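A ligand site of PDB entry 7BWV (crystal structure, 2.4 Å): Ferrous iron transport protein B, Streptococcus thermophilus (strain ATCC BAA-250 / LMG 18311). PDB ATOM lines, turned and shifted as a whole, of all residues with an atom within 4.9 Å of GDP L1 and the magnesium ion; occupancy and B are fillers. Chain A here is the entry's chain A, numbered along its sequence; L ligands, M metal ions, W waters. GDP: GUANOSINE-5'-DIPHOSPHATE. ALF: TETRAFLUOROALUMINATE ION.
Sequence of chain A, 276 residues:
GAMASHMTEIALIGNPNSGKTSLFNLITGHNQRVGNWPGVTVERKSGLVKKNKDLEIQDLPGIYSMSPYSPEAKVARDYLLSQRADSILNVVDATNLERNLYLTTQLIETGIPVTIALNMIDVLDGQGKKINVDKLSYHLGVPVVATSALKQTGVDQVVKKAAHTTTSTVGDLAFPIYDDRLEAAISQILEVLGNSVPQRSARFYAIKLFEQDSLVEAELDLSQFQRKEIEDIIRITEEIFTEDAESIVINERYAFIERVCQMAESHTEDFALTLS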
ATOM      1  N   ASN A  15     -25.621 -22.197  10.582  1.00  0.00           N
ATOM      2  CA  ASN A  15     -24.713 -21.109  10.255  1.00  0.00           C
ATOM      3  C   ASN A  15     -23.265 -21.623  10.246  1.00  0.00           C
ATOM      4  O   ASN A  15     -22.956 -22.637  10.884  1.00  0.00           O
ATOM      5  CB  ASN A  15     -24.869 -19.968  11.253  1.00  0.00           C
ATOM      6  CG  ASN A  15     -26.155 -19.183  11.068  1.00  0.00           C
ATOM      7  OD1 ASN A  15     -26.979 -19.521  10.201  1.00  0.00           O
ATOM      8  ND2 ASN A  15     -26.346 -18.139  11.867  1.00  0.00           N
ATOM      9  N   PRO A  16     -22.374 -20.942   9.521  1.00  0.00           N
ATOM     10  CA  PRO A  16     -20.956 -21.297   9.588  1.00  0.00           C
ATOM     11  C   PRO A  16     -20.422 -21.261  11.014  1.00  0.00           C
ATOM     12  O   PRO A  16     -20.864 -20.452  11.841  1.00  0.00           O
ATOM     13  CB  PRO A  16     -20.283 -20.236   8.705  1.00  0.00           C
ATOM     14  CG  PRO A  16     -21.343 -19.835   7.745  1.00  0.00           C
ATOM     15  CD  PRO A  16     -22.643 -19.911   8.507  1.00  0.00           C
ATOM     16  N   ASN A  17     -19.471 -22.150  11.296  1.00  0.00           N
ATOM     17  CA  ASN A  17     -18.753 -22.160  12.569  1.00  0.00           C
ATOM     18  C   ASN A  17     -19.674 -22.440  13.754  1.00  0.00           C
ATOM     19  O   ASN A  17     -19.389 -22.037  14.887  1.00  0.00           O
ATOM     20  CB  ASN A  17     -17.996 -20.847  12.783  1.00  0.00           C
ATOM     21  CG  ASN A  17     -16.536 -21.059  13.145  1.00  0.00           C
ATOM     22  OD1 ASN A  17     -15.987 -22.136  12.933  1.00  0.00           O
ATOM     23  ND2 ASN A  17     -15.906 -20.029  13.694  1.00  0.00           N
ATOM     24  N   SER A  18     -20.784 -23.135  13.509  1.00  0.00           N
ATOM     25  CA  SER A  18     -21.711 -23.473  14.585  1.00  0.00           C
ATOM     26  C   SER A  18     -21.399 -24.815  15.236  1.00  0.00           C
ATOM     27  O   SER A  18     -21.991 -25.143  16.265  1.00  0.00           O
ATOM     28  CB  SER A  18     -23.150 -23.470  14.059  1.00  0.00           C
ATOM     29  OG  SER A  18     -23.294 -24.338  12.944  1.00  0.00           O
ATOM     30  N   GLY A  19     -20.484 -25.599  14.656  1.00  0.00           N
ATOM     31  CA  GLY A  19     -20.134 -26.902  15.199  1.00  0.00           C
ATOM     32  C   GLY A  19     -20.701 -28.093  14.455  1.00  0.00           C
ATOM     33  O   GLY A  19     -20.795 -29.172  15.049  1.00  0.00           O
ATOM     34  N   LYS A  20     -21.076 -27.931  13.182  1.00  0.00           N
ATOM     35  CA  LYS A  20     -21.722 -29.020  12.448  1.00  0.00           C
ATOM     36  C   LYS A  20     -20.769 -30.189  12.241  1.00  0.00           C
ATOM     37  O   LYS A  20     -21.092 -31.334  12.575  1.00  0.00           O
ATOM     38  CB  LYS A  20     -22.240 -28.506  11.109  1.00  0.00           C
ATOM     39  CG  LYS A  20     -23.359 -27.468  11.220  1.00  0.00           C
ATOM     40  CD  LYS A  20     -23.841 -27.026   9.859  1.00  0.00           C
ATOM     41  CE  LYS A  20     -22.707 -26.413   9.040  1.00  0.00           C
ATOM     42  NZ  LYS A  20     -22.081 -25.234   9.719  1.00  0.00           N
ATOM     43  N   THR A  21     -19.581 -29.929  11.691  1.00  0.00           N
ATOM     44  CA  THR A  21     -18.629 -31.007  11.444  1.00  0.00           C
ATOM     45  C   THR A  21     -18.184 -31.638  12.760  1.00  0.00           C
ATOM     46  O   THR A  21     -17.949 -32.857  12.829  1.00  0.00           O
ATOM     47  CB  THR A  21     -17.423 -30.506  10.653  1.00  0.00           C
ATOM     48  OG1 THR A  21     -17.866 -29.908   9.433  1.00  0.00           O
ATOM     49  CG2 THR A  21     -16.474 -31.643  10.327  1.00  0.00           C
ATOM     50  N   SER A  22     -18.063 -30.835  13.823  1.00  0.00           N
ATOM     51  CA  SER A  22     -17.704 -31.379  15.123  1.00  0.00           C
ATOM     52  C   SER A  22     -18.745 -32.393  15.588  1.00  0.00           C
ATOM     53  O   SER A  22     -18.403 -33.470  16.091  1.00  0.00           O
ATOM     54  CB  SER A  22     -17.550 -30.268  16.153  1.00  0.00           C
ATOM     55  OG  SER A  22     -16.503 -29.375  15.806  1.00  0.00           O
ATOM     56  N   ARG A  33     -12.634 -32.328   8.629  1.00  0.00           N
ATOM     57  CA  ARG A  33     -11.903 -31.114   9.002  1.00  0.00           C
ATOM     58  C   ARG A  33     -12.760 -30.213   9.885  1.00  0.00           C
ATOM     59  O   ARG A  33     -13.867 -29.802   9.506  1.00  0.00           O
ATOM     60  CB  ARG A  33     -11.468 -30.365   7.742  1.00  0.00           C
ATOM     61  CG  ARG A  33     -10.425 -31.116   6.933  1.00  0.00           C
ATOM     62  CD  ARG A  33      -9.545 -30.170   6.136  1.00  0.00           C
ATOM     63  NE  ARG A  33      -8.303 -30.831   5.724  1.00  0.00           N
ATOM     64  CZ  ARG A  33      -7.326 -30.228   5.060  1.00  0.00           C
ATOM     65  NH1 ARG A  33      -7.437 -28.951   4.726  1.00  0.00           N
ATOM     66  NH2 ARG A  33      -6.237 -30.901   4.731  1.00  0.00           N
ATOM     67  N   VAL A  34     -12.232 -29.905  11.074  1.00  0.00           N
ATOM     68  CA  VAL A  34     -12.858 -28.985  12.029  1.00  0.00           C
ATOM     69  C   VAL A  34     -11.876 -27.842  12.255  1.00  0.00           C
ATOM     70  O   VAL A  34     -10.688 -28.078  12.526  1.00  0.00           O
ATOM     71  CB  VAL A  34     -13.202 -29.694  13.348  1.00  0.00           C
ATOM     72  CG1 VAL A  34     -13.677 -28.691  14.395  1.00  0.00           C
ATOM     73  CG2 VAL A  34     -14.252 -30.774  13.113  1.00  0.00           C
ATOM     74  N   GLY A  35     -12.375 -26.609  12.169  1.00  0.00           N
ATOM     75  CA  GLY A  35     -11.527 -25.439  12.355  1.00  0.00           C
ATOM     76  C   GLY A  35     -12.293 -24.305  12.989  1.00  0.00           C
ATOM     77  O   GLY A  35     -13.489 -24.114  12.726  1.00  0.00           O
ATOM     78  N   ASN A  36     -11.603 -23.522  13.824  1.00  0.00           N
ATOM     79  CA  ASN A  36     -12.240 -22.436  14.555  1.00  0.00           C
ATOM     80  C   ASN A  36     -12.336 -21.162  13.709  1.00  0.00           C
ATOM     81  O   ASN A  36     -12.002 -20.073  14.172  1.00  0.00           O
ATOM     82  CB  ASN A  36     -11.485 -22.142  15.858  1.00  0.00           C
ATOM     83  CG  ASN A  36     -10.034 -21.771  15.629  1.00  0.00           C
ATOM     84  OD1 ASN A  36      -9.465 -22.028  14.566  1.00  0.00           O
ATOM     85  ND2 ASN A  36      -9.417 -21.150  16.630  1.00  0.00           N
ATOM     86  N   THR A  41     -15.685 -26.494   5.939  1.00  0.00           N
ATOM     87  CA  THR A  41     -16.420 -27.426   5.101  1.00  0.00           C
ATOM     88  C   THR A  41     -16.950 -26.703   3.864  1.00  0.00           C
ATOM     89  O   THR A  41     -17.661 -25.693   3.985  1.00  0.00           O
ATOM     90  CB  THR A  41     -17.572 -28.048   5.883  1.00  0.00           C
ATOM     91  OG1 THR A  41     -17.066 -28.634   7.086  1.00  0.00           O
ATOM     92  CG2 THR A  41     -18.272 -29.118   5.048  1.00  0.00           C
ATOM     93  N   ASP A  59     -22.876 -34.058   6.498  1.00  0.00           N
ATOM     94  CA  ASP A  59     -22.223 -32.813   6.842  1.00  0.00           C
ATOM     95  C   ASP A  59     -22.273 -31.864   5.651  1.00  0.00           C
ATOM     96  O   ASP A  59     -22.020 -32.269   4.510  1.00  0.00           O
ATOM     97  CB  ASP A  59     -20.763 -33.068   7.256  1.00  0.00           C
ATOM     98  CG  ASP A  59     -20.126 -31.867   7.933  1.00  0.00           C
ATOM     99  OD1 ASP A  59     -20.847 -31.020   8.494  1.00  0.00           O
ATOM    100  OD2 ASP A  59     -18.875 -31.772   7.910  1.00  0.00           O
ATOM    101  N   LEU A  60     -22.597 -30.605   5.911  1.00  0.00           N
ATOM    102  CA  LEU A  60     -22.817 -29.645   4.836  1.00  0.00           C
ATOM    103  C   LEU A  60     -22.166 -28.314   5.191  1.00  0.00           C
ATOM    104  O   LEU A  60     -21.986 -28.010   6.383  1.00  0.00           O
ATOM    105  CB  LEU A  60     -24.314 -29.445   4.558  1.00  0.00           C
ATOM    106  CG  LEU A  60     -24.938 -30.630   3.815  1.00  0.00           C
ATOM    107  CD1 LEU A  60     -26.405 -30.780   4.138  1.00  0.00           C
ATOM    108  CD2 LEU A  60     -24.720 -30.482   2.310  1.00  0.00           C
ATOM    109  N   ASN A 119     -26.269 -26.032  20.003  1.00  0.00           N
ATOM    110  CA  ASN A 119     -24.889 -26.419  20.233  1.00  0.00           C
ATOM    111  C   ASN A 119     -24.102 -25.307  20.927  1.00  0.00           C
ATOM    112  O   ASN A 119     -24.568 -24.174  21.085  1.00  0.00           O
ATOM    113  CB  ASN A 119     -24.225 -26.793  18.907  1.00  0.00           C
ATOM    114  CG  ASN A 119     -22.968 -27.627  19.095  1.00  0.00           C
ATOM    115  OD1 ASN A 119     -22.942 -28.536  19.934  1.00  0.00           O
ATOM    116  ND2 ASN A 119     -21.928 -27.309  18.341  1.00  0.00           N
ATOM    117  N   MET A 120     -22.883 -25.659  21.343  1.00  0.00           N
ATOM    118  CA  MET A 120     -22.000 -24.757  22.088  1.00  0.00           C
ATOM    119  C   MET A 120     -22.664 -24.251  23.363  1.00  0.00           C
ATOM    120  O   MET A 120     -22.445 -23.108  23.785  1.00  0.00           O
ATOM    121  CB  MET A 120     -21.531 -23.588  21.223  1.00  0.00           C
ATOM    122  CG  MET A 120     -21.144 -23.977  19.797  1.00  0.00           C
ATOM    123  SD  MET A 120     -20.130 -22.745  18.950  1.00  0.00           S
ATOM    124  CE  MET A 120     -19.218 -22.043  20.313  1.00  0.00           C
ATOM    125  N   ILE A 121     -23.474 -25.102  23.998  1.00  0.00           N
ATOM    126  CA  ILE A 121     -24.144 -24.724  25.229  1.00  0.00           C
ATOM    127  C   ILE A 121     -23.145 -24.594  26.382  1.00  0.00           C
ATOM    128  O   ILE A 121     -23.436 -23.899  27.369  1.00  0.00           O
ATOM    129  CB  ILE A 121     -25.262 -25.721  25.557  1.00  0.00           C
ATOM    130  CG1 ILE A 121     -26.244 -25.119  26.562  1.00  0.00           C
ATOM    131  CG2 ILE A 121     -24.694 -27.031  26.089  1.00  0.00           C
ATOM    132  CD1 ILE A 121     -27.145 -24.058  25.955  1.00  0.00           C
ATOM    133  N   ASP A 122     -21.986 -25.235  26.284  1.00  0.00           N
ATOM    134  CA  ASP A 122     -20.965 -25.089  27.310  1.00  0.00           C
ATOM    135  C   ASP A 122     -20.409 -23.673  27.342  1.00  0.00           C
ATOM    136  O   ASP A 122     -20.005 -23.184  28.404  1.00  0.00           O
ATOM    137  CB  ASP A 122     -19.837 -26.097  27.083  1.00  0.00           C
ATOM    138  CG  ASP A 122     -19.232 -25.991  25.697  1.00  0.00           C
ATOM    139  OD1 ASP A 122     -19.905 -26.367  24.715  1.00  0.00           O
ATOM    140  OD2 ASP A 122     -18.079 -25.520  25.581  1.00  0.00           O
ATOM    141  N   VAL A 123     -20.372 -23.002  26.183  1.00  0.00           N
ATOM    142  CA  VAL A 123     -19.905 -21.623  26.146  1.00  0.00           C
ATOM    143  C   VAL A 123     -20.878 -20.723  26.891  1.00  0.00           C
ATOM    144  O   VAL A 123     -20.463 -19.855  27.671  1.00  0.00           O
ATOM    145  CB  VAL A 123     -19.715 -21.159  24.683  1.00  0.00           C
ATOM    146  CG1 VAL A 123     -19.260 -19.714  24.650  1.00  0.00           C
ATOM    147  CG2 VAL A 123     -18.726 -22.063  23.972  1.00  0.00           C
ATOM    148  N   THR A 147     -26.830 -29.221  23.108  1.00  0.00           N
ATOM    149  CA  THR A 147     -25.692 -30.089  22.823  1.00  0.00           C
ATOM    150  C   THR A 147     -24.382 -29.350  23.035  1.00  0.00           C
ATOM    151  O   THR A 147     -24.303 -28.128  22.956  1.00  0.00           O
ATOM    152  CB  THR A 147     -25.728 -30.639  21.389  1.00  0.00           C
ATOM    153  OG1 THR A 147     -25.545 -29.559  20.455  1.00  0.00           O
ATOM    154  CG2 THR A 147     -27.050 -31.341  21.100  1.00  0.00           C
ATOM    155  N   SER A 148     -23.342 -30.133  23.319  1.00  0.00           N
ATOM    156  CA  SER A 148     -21.962 -29.654  23.376  1.00  0.00           C
ATOM    157  C   SER A 148     -21.098 -30.651  22.627  1.00  0.00           C
ATOM    158  O   SER A 148     -20.963 -31.806  23.070  1.00  0.00           O
ATOM    159  CB  SER A 148     -21.487 -29.475  24.815  1.00  0.00           C
ATOM    160  OG  SER A 148     -20.352 -28.629  24.873  1.00  0.00           O
ATOM    161  N   ALA A 149     -20.536 -30.248  21.496  1.00  0.00           N
ATOM    162  CA  ALA A 149     -19.601 -31.118  20.793  1.00  0.00           C
ATOM    163  C   ALA A 149     -18.265 -31.207  21.518  1.00  0.00           C
ATOM    164  O   ALA A 149     -17.546 -32.197  21.372  1.00  0.00           O
ATOM    165  CB  ALA A 149     -19.398 -30.634  19.358  1.00  0.00           C
ATOM    166  N   LEU A 150     -17.918 -30.176  22.294  1.00  0.00           N
ATOM    167  CA  LEU A 150     -16.674 -30.213  23.056  1.00  0.00           C
ATOM    168  C   LEU A 150     -16.796 -31.145  24.258  1.00  0.00           C
ATOM    169  O   LEU A 150     -16.016 -32.078  24.422  1.00  0.00           O
ATOM    170  CB  LEU A 150     -16.300 -28.800  23.502  1.00  0.00           C
ATOM    171  CG  LEU A 150     -14.890 -28.614  24.079  1.00  0.00           C
ATOM    172  CD1 LEU A 150     -13.924 -28.244  22.977  1.00  0.00           C
ATOM    173  CD2 LEU A 150     -14.883 -27.575  25.189  1.00  0.00           C
HETATM  174  PB  GDP L   1     -18.958 -25.964  11.321  1.00  0.00           P
HETATM  175  O1B GDP L   1     -20.372 -25.799  11.816  1.00  0.00           O
HETATM  176  O2B GDP L   1     -18.643 -27.307  10.671  1.00  0.00           O
HETATM  177  O3B GDP L   1     -18.317 -24.738  10.713  1.00  0.00           O
HETATM  178  O3A GDP L   1     -17.974 -25.920  12.712  1.00  0.00           O
HETATM  179  PA  GDP L   1     -16.874 -26.917  13.081  1.00  0.00           P
HETATM  180  O1A GDP L   1     -17.226 -28.213  13.717  1.00  0.00           O
HETATM  181  O2A GDP L   1     -15.562 -26.772  12.358  1.00  0.00           O
HETATM  182  O5' GDP L   1     -16.343 -26.097  14.638  1.00  0.00           O
HETATM  183  C5' GDP L   1     -15.973 -24.816  14.568  1.00  0.00           C
HETATM  184  C4' GDP L   1     -15.273 -24.470  15.947  1.00  0.00           C
HETATM  185  O4' GDP L   1     -16.228 -24.561  16.994  1.00  0.00           O
HETATM  186  C3' GDP L   1     -14.125 -25.467  16.293  1.00  0.00           C
HETATM  187  O3' GDP L   1     -13.132 -24.721  16.917  1.00  0.00           O
HETATM  188  C2' GDP L   1     -14.792 -26.421  17.299  1.00  0.00           C
HETATM  189  O2' GDP L   1     -13.933 -26.950  18.250  1.00  0.00           O
HETATM  190  C1' GDP L   1     -15.743 -25.411  18.012  1.00  0.00           C
HETATM  191  N9  GDP L   1     -16.905 -26.107  18.553  1.00  0.00           N
HETATM  192  C8  GDP L   1     -17.793 -26.999  17.904  1.00  0.00           C
HETATM  193  N7  GDP L   1     -18.751 -27.451  18.735  1.00  0.00           N
HETATM  194  C5  GDP L   1     -18.480 -26.825  19.952  1.00  0.00           C
HETATM  195  C6  GDP L   1     -19.195 -26.951  21.185  1.00  0.00           C
HETATM  196  O6  GDP L   1     -20.186 -27.604  21.467  1.00  0.00           O
HETATM  197  N1  GDP L   1     -18.617 -26.160  22.230  1.00  0.00           N
HETATM  198  C2  GDP L   1     -17.478 -25.361  22.025  1.00  0.00           C
HETATM  199  N2  GDP L   1     -17.011 -24.636  23.116  1.00  0.00           N
HETATM  200  N3  GDP L   1     -16.782 -25.233  20.872  1.00  0.00           N
HETATM  201  C4  GDP L   1     -17.340 -25.998  19.859  1.00  0.00           C
HETATM  202 AL   ALF L   2     -18.178 -24.378   8.459  1.00  0.00          AL
HETATM  203  F1  ALF L   2     -18.248 -26.001   8.304  1.00  0.00           F
HETATM  204  F2  ALF L   2     -18.104 -22.753   8.636  1.00  0.00           F
HETATM  205  F3  ALF L   2     -19.826 -24.319   8.441  1.00  0.00           F
HETATM  206  F4  ALF L   2     -16.555 -24.478   8.451  1.00  0.00           F
HETATM  207 MG    MG M   1     -17.966 -27.855   8.759  1.00  0.00          MG
HETATM  208  O   HOH W   1     -15.916 -27.735   9.762  1.00  0.00           O
HETATM  209  O   HOH W   2     -20.089 -28.299   8.302  1.00  0.00           O
HETATM  210  O   HOH W   3     -10.781 -25.945  16.385  1.00  0.00           O
HETATM  211  O   HOH W   4     -13.876 -22.674  18.663  1.00  0.00           O
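O2B of GDP L1 lies close to N of Thr 21, 3.0 Å away.
OG of Ser 22 is in hydrogen-bond range of O1A of GDP L1 (2.5 Å).
An oxygen (O6) of GDP L1 is in hydrogen-bond range of the backbone NH of Met 120 (3.3 Å).
N of Ala 149 is in hydrogen-bond range of O6 of GDP L1, 2.7 Å away.
OG of Ser 18 is in hydrogen-bond range of O1B of GDP L1 (3.5 Å).
The backbone NH (N) of Asn 17 is in hydrogen-bond range of a fluorine (F2) of ALF L2 (3.1 Å).
OD1 of Asp 122 is in hydrogen-bond range of N1 of GDP L1, at 2.8 Å.
N7 of GDP L1 is in hydrogen-bond range of ND2 of Asn 119 (3.2 Å).
N of Gly 35 is in hydrogen-bond range of O2A of GDP L1, at 3.2 Å.
N of Ser 18 is in hydrogen-bond range of O1B of GDP L1, at 3.2 Å.
The backbone NH (N) of Thr 41 is in hydrogen-bond range of a fluorine (F4) of ALF L2 (3.3 Å).
The backbone NH of Gly 19 is in hydrogen-bond range of an oxygen (O1B) of GDP L1, 2.8 Å away.
N of Lys 20 is in hydrogen-bond range of O1B of GDP L1, 2.6 Å away.
N of Ser 22 is in hydrogen-bond range of O1A of GDP L1.
The side-chain amino group (NZ) of Lys 20 is in hydrogen-bond range of a fluorine (F3) of ALF L2.
The backbone NH of Asn 17 sits close to an oxygen (O3B) of GDP L1, 2.9 Å away.
The side-chain amino group (NZ) of Lys 20 lies within salt-bridge range of an oxygen (O1B) of GDP L1, 2.8 Å away.
An aluminium atom (AL) of ALF L2 is bound by an oxygen (O3B) of GDP L1, at 2.3 Å.
The backbone carbonyl oxygen (O) of Thr 147 lies within hydrogen-bond range of the backbone NH (N) of Met 120 (3.3 Å).
The side-chain amide oxygen (OD1) of Asn 119 is in hydrogen-bond range of the side-chain hydroxyl (OG1) of Thr 147 (2.8 Å).
OD1 of Asn 17 sits close to O of Gly 35 (3.2 Å).
O of Asn 15 sits at hydrogen-bond distance from OG of Ser 18 (2.7 Å).
The backbone carbonyl oxygen of Ser 18 sits at hydrogen-bond distance from the side-chain amide nitrogen of Asn 119 (3.0 Å).
NZ of Lys 20 sits at hydrogen-bond distance from O of Asn 15 (3.0 Å).
OD1 of Asn 119 lies within hydrogen-bond range of N of Ala 149, 3.3 Å away.
OG1 of Thr 21 sits close to OD2 of Asp 59 (2.6 Å).
Val 34 touches GDP L1 (CG1 to O2A, 3.4 Å).
Asn 36 touches GDP L1.
CG2 of Val 123 touches N2 of GDP L1, 3.2 Å away.
Ser 148 touches GDP L1.
N of Leu 150 touches O6 of GDP L1 (3.5 Å).
Hydrophobic or aromatic side chains within 4 Å of GDP L1: Val 34, Met 120, Val 123, Ala 149 and Leu 150.
Of the 24 residues printed, 2 come within 4 Å of the magnesium ion.
The magnesium ion is bound by a fluorine (F1) of ALF L2, the side-chain hydroxyl of Thr 41, an oxygen (O2B) of GDP L1, the side-chain hydroxyl of Thr 21, water W2 and water W1.
The magnesium ion has six donor atoms within binding distance.
Water W2 lies within hydrogen-bond range of the backbone carbonyl oxygen (O) of Leu 60 (2.7 Å) and the side-chain carboxylate (OD1) of Asp 59 (2.8 Å).
Water W1 bridges an oxygen (O2A) of GDP L1 (2.8 Å) and the backbone carbonyl oxygen of Arg 33 (2.9 Å).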
